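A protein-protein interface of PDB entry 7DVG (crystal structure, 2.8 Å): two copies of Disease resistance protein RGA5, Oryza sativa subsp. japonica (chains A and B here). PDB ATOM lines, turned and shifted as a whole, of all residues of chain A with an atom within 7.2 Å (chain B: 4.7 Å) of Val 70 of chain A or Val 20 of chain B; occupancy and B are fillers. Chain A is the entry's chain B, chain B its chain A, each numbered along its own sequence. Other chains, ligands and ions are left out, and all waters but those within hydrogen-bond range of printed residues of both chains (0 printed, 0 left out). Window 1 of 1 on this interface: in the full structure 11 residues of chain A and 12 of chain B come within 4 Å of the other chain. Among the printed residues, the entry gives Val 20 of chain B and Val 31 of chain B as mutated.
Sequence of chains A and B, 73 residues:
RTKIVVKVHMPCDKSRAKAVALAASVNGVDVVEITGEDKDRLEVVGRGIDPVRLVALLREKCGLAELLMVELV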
ATOM      1  N   THR A   2     -14.304  23.323   6.986  1.00  0.00           N
ATOM      2  CA  THR A   2     -15.222  22.388   7.640  1.00  0.00           C
ATOM      3  C   THR A   2     -14.615  21.760   8.892  1.00  0.00           C
ATOM      4  O   THR A   2     -13.461  21.318   8.881  1.00  0.00           O
ATOM      5  CB  THR A   2     -15.670  21.277   6.672  1.00  0.00           C
ATOM      6  OG1 THR A   2     -16.365  20.267   7.410  1.00  0.00           O
ATOM      7  CG2 THR A   2     -14.480  20.644   5.935  1.00  0.00           C
ATOM      8  N   LYS A   3     -15.411  21.702   9.962  1.00  0.00           N
ATOM      9  CA  LYS A   3     -15.000  21.159  11.254  1.00  0.00           C
ATOM     10  C   LYS A   3     -15.929  20.019  11.644  1.00  0.00           C
ATOM     11  O   LYS A   3     -17.159  20.135  11.513  1.00  0.00           O
ATOM     12  CB  LYS A   3     -15.027  22.245  12.326  1.00  0.00           C
ATOM     13  CG  LYS A   3     -15.513  21.791  13.680  1.00  0.00           C
ATOM     14  CD  LYS A   3     -15.174  22.828  14.736  1.00  0.00           C
ATOM     15  CE  LYS A   3     -16.205  22.847  15.868  1.00  0.00           C
ATOM     16  NZ  LYS A   3     -15.705  23.542  17.097  1.00  0.00           N
ATOM     17  N   ILE A   4     -15.347  18.906  12.104  1.00  0.00           N
ATOM     18  CA  ILE A   4     -16.138  17.735  12.466  1.00  0.00           C
ATOM     19  C   ILE A   4     -15.632  17.154  13.779  1.00  0.00           C
ATOM     20  O   ILE A   4     -14.479  17.344  14.171  1.00  0.00           O
ATOM     21  CB  ILE A   4     -16.129  16.643  11.378  1.00  0.00           C
ATOM     22  CG1 ILE A   4     -14.945  15.720  11.599  1.00  0.00           C
ATOM     23  CG2 ILE A   4     -16.094  17.242   9.966  1.00  0.00           C
ATOM     24  CD1 ILE A   4     -14.920  14.606  10.643  1.00  0.00           C
ATOM     25  N   VAL A   5     -16.523  16.431  14.456  1.00  0.00           N
ATOM     26  CA  VAL A   5     -16.284  15.945  15.809  1.00  0.00           C
ATOM     27  C   VAL A   5     -16.627  14.468  15.873  1.00  0.00           C
ATOM     28  O   VAL A   5     -17.781  14.083  15.639  1.00  0.00           O
ATOM     29  CB  VAL A   5     -17.102  16.720  16.846  1.00  0.00           C
ATOM     30  CG1 VAL A   5     -16.989  16.026  18.190  1.00  0.00           C
ATOM     31  CG2 VAL A   5     -16.595  18.148  16.932  1.00  0.00           C
ATOM     32  N   PRO A  51     -15.960  12.776   5.670  1.00  0.00           N
ATOM     33  CA  PRO A  51     -16.213  12.389   7.072  1.00  0.00           C
ATOM     34  C   PRO A  51     -16.252  10.891   7.253  1.00  0.00           C
ATOM     35  O   PRO A  51     -15.706  10.378   8.240  1.00  0.00           O
ATOM     36  CB  PRO A  51     -17.554  13.072   7.402  1.00  0.00           C
ATOM     37  CG  PRO A  51     -17.873  13.965   6.195  1.00  0.00           C
ATOM     38  CD  PRO A  51     -17.148  13.353   5.026  1.00  0.00           C
ATOM     39  N   LEU A  67     -19.608   9.604  14.300  1.00  0.00           N
ATOM     40  CA  LEU A  67     -19.619  10.984  13.846  1.00  0.00           C
ATOM     41  C   LEU A  67     -20.733  11.742  14.560  1.00  0.00           C
ATOM     42  O   LEU A  67     -21.917  11.434  14.382  1.00  0.00           O
ATOM     43  CB  LEU A  67     -19.813  11.020  12.341  1.00  0.00           C
ATOM     44  CG  LEU A  67     -19.927  12.394  11.721  1.00  0.00           C
ATOM     45  CD1 LEU A  67     -18.970  13.381  12.347  1.00  0.00           C
ATOM     46  CD2 LEU A  67     -19.676  12.249  10.254  1.00  0.00           C
ATOM     47  N   LEU A  68     -20.351  12.750  15.344  1.00  0.00           N
ATOM     48  CA  LEU A  68     -21.276  13.480  16.206  1.00  0.00           C
ATOM     49  C   LEU A  68     -21.816  14.747  15.553  1.00  0.00           C
ATOM     50  O   LEU A  68     -23.025  15.011  15.605  1.00  0.00           O
ATOM     51  CB  LEU A  68     -20.590  13.850  17.522  1.00  0.00           C
ATOM     52  CG  LEU A  68     -20.609  12.863  18.684  1.00  0.00           C
ATOM     53  CD1 LEU A  68     -20.470  11.413  18.223  1.00  0.00           C
ATOM     54  CD2 LEU A  68     -19.500  13.257  19.645  1.00  0.00           C
ATOM     55  N   MET A  69     -20.935  15.560  14.972  1.00  0.00           N
ATOM     56  CA  MET A  69     -21.383  16.758  14.281  1.00  0.00           C
ATOM     57  C   MET A  69     -20.400  17.099  13.172  1.00  0.00           C
ATOM     58  O   MET A  69     -19.235  16.692  13.199  1.00  0.00           O
ATOM     59  CB  MET A  69     -21.537  17.953  15.230  1.00  0.00           C
ATOM     60  CG  MET A  69     -20.245  18.695  15.463  1.00  0.00           C
ATOM     61  SD  MET A  69     -20.481  20.388  16.027  1.00  0.00           S
ATOM     62  CE  MET A  69     -19.194  20.495  17.283  1.00  0.00           C
ATOM     63  N   VAL A  70     -20.893  17.843  12.183  1.00  0.00           N
ATOM     64  CA  VAL A  70     -20.051  18.446  11.155  1.00  0.00           C
ATOM     65  C   VAL A  70     -20.552  19.867  10.907  1.00  0.00           C
ATOM     66  O   VAL A  70     -21.758  20.090  10.748  1.00  0.00           O
ATOM     67  CB  VAL A  70     -20.047  17.623   9.855  1.00  0.00           C
ATOM     68  CG1 VAL A  70     -21.407  17.282   9.494  1.00  0.00           C
ATOM     69  CG2 VAL A  70     -19.457  18.425   8.738  1.00  0.00           C
ATOM     70  N   GLU A  71     -19.627  20.829  10.880  1.00  0.00           N
ATOM     71  CA  GLU A  71     -19.973  22.244  10.860  1.00  0.00           C
ATOM     72  C   GLU A  71     -19.225  22.954   9.739  1.00  0.00           C
ATOM     73  O   GLU A  71     -18.047  22.674   9.495  1.00  0.00           O
ATOM     74  CB  GLU A  71     -19.657  22.856  12.224  1.00  0.00           C
ATOM     75  CG  GLU A  71     -19.518  24.355  12.276  1.00  0.00           C
ATOM     76  CD  GLU A  71     -19.515  24.865  13.714  1.00  0.00           C
ATOM     77  OE1 GLU A  71     -19.470  24.028  14.649  1.00  0.00           O
ATOM     78  OE2 GLU A  71     -19.547  26.100  13.910  1.00  0.00           O
ATOM     79  N   LEU A  72     -19.921  23.857   9.035  1.00  0.00           N
ATOM     80  CA  LEU A  72     -19.349  24.609   7.911  1.00  0.00           C
ATOM     81  C   LEU A  72     -19.021  26.027   8.383  1.00  0.00           C
ATOM     82  O   LEU A  72     -19.889  26.903   8.384  1.00  0.00           O
ATOM     83  CB  LEU A  72     -20.308  24.638   6.721  1.00  0.00           C
ATOM     84  CG  LEU A  72     -20.153  23.605   5.593  1.00  0.00           C
ATOM     85  CD1 LEU A  72     -18.806  23.780   4.876  1.00  0.00           C
ATOM     86  CD2 LEU A  72     -20.319  22.166   6.068  1.00  0.00           C
ATOM     87  N   ARG B  16     -24.762   6.480   9.558  1.00  0.00           N
ATOM     88  CA  ARG B  16     -24.804   7.745  10.287  1.00  0.00           C
ATOM     89  C   ARG B  16     -23.895   8.755   9.618  1.00  0.00           C
ATOM     90  O   ARG B  16     -24.330   9.858   9.270  1.00  0.00           O
ATOM     91  CB  ARG B  16     -24.393   7.549  11.747  1.00  0.00           C
ATOM     92  CG  ARG B  16     -25.540   7.566  12.735  1.00  0.00           C
ATOM     93  CD  ARG B  16     -25.044   7.279  14.149  1.00  0.00           C
ATOM     94  NE  ARG B  16     -25.092   5.850  14.464  1.00  0.00           N
ATOM     95  CZ  ARG B  16     -26.190   5.186  14.816  1.00  0.00           C
ATOM     96  NH1 ARG B  16     -27.347   5.819  14.911  1.00  0.00           N
ATOM     97  NH2 ARG B  16     -26.126   3.887  15.079  1.00  0.00           N
ATOM     98  N   ALA B  17     -22.627   8.365   9.402  1.00  0.00           N
ATOM     99  CA  ALA B  17     -21.635   9.265   8.830  1.00  0.00           C
ATOM    100  C   ALA B  17     -22.097   9.808   7.487  1.00  0.00           C
ATOM    101  O   ALA B  17     -22.078  11.023   7.260  1.00  0.00           O
ATOM    102  CB  ALA B  17     -20.299   8.544   8.680  1.00  0.00           C
ATOM    103  N   LYS B  18     -22.548   8.927   6.588  1.00  0.00           N
ATOM    104  CA  LYS B  18     -22.884   9.409   5.252  1.00  0.00           C
ATOM    105  C   LYS B  18     -24.189  10.192   5.236  1.00  0.00           C
ATOM    106  O   LYS B  18     -24.337  11.111   4.424  1.00  0.00           O
ATOM    107  CB  LYS B  18     -22.927   8.255   4.257  1.00  0.00           C
ATOM    108  CG  LYS B  18     -23.793   7.131   4.671  1.00  0.00           C
ATOM    109  CD  LYS B  18     -23.556   5.922   3.786  1.00  0.00           C
ATOM    110  CE  LYS B  18     -22.148   5.870   3.248  1.00  0.00           C
ATOM    111  NZ  LYS B  18     -22.054   4.822   2.205  1.00  0.00           N
ATOM    112  N   ALA B  19     -25.119   9.885   6.140  1.00  0.00           N
ATOM    113  CA  ALA B  19     -26.288  10.748   6.297  1.00  0.00           C
ATOM    114  C   ALA B  19     -25.881  12.111   6.851  1.00  0.00           C
ATOM    115  O   ALA B  19     -26.238  13.151   6.277  1.00  0.00           O
ATOM    116  CB  ALA B  19     -27.333  10.085   7.199  1.00  0.00           C
ATOM    117  N   VAL B  20     -25.136  12.127   7.971  1.00  0.00           N
ATOM    118  CA  VAL B  20     -24.654  13.404   8.497  1.00  0.00           C
ATOM    119  C   VAL B  20     -23.965  14.179   7.364  1.00  0.00           C
ATOM    120  O   VAL B  20     -24.136  15.401   7.243  1.00  0.00           O
ATOM    121  CB  VAL B  20     -23.725  13.216   9.748  1.00  0.00           C
ATOM    122  CG1 VAL B  20     -23.251  14.526  10.230  1.00  0.00           C
ATOM    123  CG2 VAL B  20     -24.411  12.591  10.977  1.00  0.00           C
ATOM    124  N   ALA B  21     -23.261  13.478   6.459  1.00  0.00           N
ATOM    125  CA  ALA B  21     -22.501  14.174   5.411  1.00  0.00           C
ATOM    126  C   ALA B  21     -23.373  14.657   4.264  1.00  0.00           C
ATOM    127  O   ALA B  21     -23.031  15.653   3.621  1.00  0.00           O
ATOM    128  CB  ALA B  21     -21.395  13.288   4.835  1.00  0.00           C
ATOM    129  N   LEU B  22     -24.466  13.958   3.958  1.00  0.00           N
ATOM    130  CA  LEU B  22     -25.333  14.429   2.888  1.00  0.00           C
ATOM    131  C   LEU B  22     -25.971  15.757   3.272  1.00  0.00           C
ATOM    132  O   LEU B  22     -25.813  16.762   2.566  1.00  0.00           O
ATOM    133  CB  LEU B  22     -26.397  13.380   2.576  1.00  0.00           C
ATOM    134  CG  LEU B  22     -26.989  13.360   1.171  1.00  0.00           C
ATOM    135  CD1 LEU B  22     -25.961  12.870   0.185  1.00  0.00           C
ATOM    136  CD2 LEU B  22     -28.205  12.459   1.147  1.00  0.00           C
ATOM    137  N   ALA B  23     -26.665  15.787   4.414  1.00  0.00           N
ATOM    138  CA  ALA B  23     -27.267  17.027   4.898  1.00  0.00           C
ATOM    139  C   ALA B  23     -26.250  18.160   4.959  1.00  0.00           C
ATOM    140  O   ALA B  23     -26.582  19.320   4.680  1.00  0.00           O
ATOM    141  CB  ALA B  23     -27.880  16.808   6.280  1.00  0.00           C
ATOM    142  N   ALA B  24     -25.003  17.846   5.325  1.00  0.00           N
ATOM    143  CA  ALA B  24     -23.994  18.897   5.380  1.00  0.00           C
ATOM    144  C   ALA B  24     -23.853  19.602   4.034  1.00  0.00           C
ATOM    145  O   ALA B  24     -23.609  20.817   3.990  1.00  0.00           O
ATOM    146  CB  ALA B  24     -22.651  18.321   5.841  1.00  0.00           C
ATOM    147  N   ASP B  30     -25.507  25.157   7.866  1.00  0.00           N
ATOM    148  CA  ASP B  30     -24.331  25.552   8.631  1.00  0.00           C
ATOM    149  C   ASP B  30     -23.781  24.415   9.484  1.00  0.00           C
ATOM    150  O   ASP B  30     -22.565  24.347   9.695  1.00  0.00           O
ATOM    151  CB  ASP B  30     -24.665  26.732   9.550  1.00  0.00           C
ATOM    152  CG  ASP B  30     -25.004  28.009   8.785  1.00  0.00           C
ATOM    153  OD1 ASP B  30     -24.396  28.266   7.716  1.00  0.00           O
ATOM    154  OD2 ASP B  30     -25.875  28.768   9.273  1.00  0.00           O
ATOM    155  N   VAL B  31     -24.638  23.517   9.973  1.00  0.00           N
ATOM    156  CA  VAL B  31     -24.189  22.480  10.898  1.00  0.00           C
ATOM    157  C   VAL B  31     -25.192  21.335  10.916  1.00  0.00           C
ATOM    158  O   VAL B  31     -26.409  21.538  10.814  1.00  0.00           O
ATOM    159  CB  VAL B  31     -23.979  23.049  12.319  1.00  0.00           C
ATOM    160  CG1 VAL B  31     -25.280  23.557  12.865  1.00  0.00           C
ATOM    161  CG2 VAL B  31     -23.449  21.966  13.239  1.00  0.00           C
ATOM    162  N   VAL B  32     -24.661  20.129  11.068  1.00  0.00           N
ATOM    163  CA  VAL B  32     -25.451  18.921  11.249  1.00  0.00           C
ATOM    164  C   VAL B  32     -24.928  18.198  12.485  1.00  0.00           C
ATOM    165  O   VAL B  32     -23.717  18.173  12.731  1.00  0.00           O
ATOM    166  CB  VAL B  32     -25.367  18.013  10.006  1.00  0.00           C
ATOM    167  CG1 VAL B  32     -26.259  16.781  10.169  1.00  0.00           C
ATOM    168  CG2 VAL B  32     -25.765  18.804   8.763  1.00  0.00           C
ATOM    169  N   LEU B  42     -31.218  13.390  12.817  1.00  0.00           N
ATOM    170  CA  LEU B  42     -30.292  14.486  12.584  1.00  0.00           C
ATOM    171  C   LEU B  42     -30.950  15.808  12.938  1.00  0.00           C
ATOM    172  O   LEU B  42     -32.164  15.989  12.779  1.00  0.00           O
ATOM    173  CB  LEU B  42     -29.808  14.519  11.136  1.00  0.00           C
ATOM    174  CG  LEU B  42     -29.226  13.223  10.610  1.00  0.00           C
ATOM    175  CD1 LEU B  42     -29.005  13.314   9.083  1.00  0.00           C
ATOM    176  CD2 LEU B  42     -27.929  12.975  11.390  1.00  0.00           C
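The backbone carbonyl oxygen (O) of Asp 30 of chain B is in hydrogen-bond range of the backbone NH (N) of Leu 72 of chain A. The backbone NH (N) of Val 70 of chain A lies within hydrogen-bond range of the backbone carbonyl oxygen (O) of Val 32 of chain B, 2.9 Å away.
The backbone NH of Glu 71 of chain A lies within hydrogen-bond range of the backbone carbonyl oxygen of Lys 3 of chain A (2.6 Å). N of Val 5 of chain A sits at hydrogen-bond distance from O of Met 69 of chain A, at 3.0 Å.
Among the printed residues, pairs that only touch across the chains: Met 69 of chain A with Val 32 of chain B (3.1 Å), Val 70 of chain A with Val 20 of chain B (3.4 Å), Val 70 of chain A with Val 31 of chain B (3.4 Å), Glu 71 of chain A with Asp 30 of chain B (3.5 Å), Pro 51 of chain A with Ala 21 of chain B (3.8 Å), Leu 67 of chain A with Ala 17 of chain B (3.8 Å) and Val 70 of chain A with Ala 24 of chain B (3.996 Å).
Printed residues of chain B within 4 Å of Val 70 of chain A: Val 20 (3.4 Å), Ala 24 (3.996 Å), Val 31 (3.4 Å) and Val 32 (2.9 Å). Val 20 of chain B touches one residue of chain A. Of the printed residues of chain B, Leu 67 of chain A touches Ala 17. Of the printed residues of chain A, Val 32 of chain B touches Met 69 (3.1 Å) and Val 70 (2.9 Å). The nearest printed residue of chain B that does not touch Val 70 of chain A is Asp 30 of chain B (4.5 Å). The nearest printed residue of chain A that does not touch Ala 24 of chain B is Leu 72 of chain A (4.1 Å).
Of the 13 printed residues of chain B, 7 touch a printed residue of chain A. Hydrophobic or aromatic side chains of chain B that line the printed part of chain A: Val 20, Ala 21, Ala 24 and Val 31. Printed residues of chain A that touch a printed residue of chain B: Pro 51, Leu 67, Met 69, Val 70, Glu 71 and Leu 72. Along chain A the printed residues that touch a printed residue of chain B span positions 51 to 72. Among the printed residues, 9 pairs touch across the chains. Among the printed residues, no Asp or Glu carboxylate lies within 4 Å of a Lys or Arg side-chain nitrogen of the other chain.
No position is printed for both chains. Of the 9 pairs that touch across the chains among the printed residues, none has its exchanged pair printed and touching as well.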
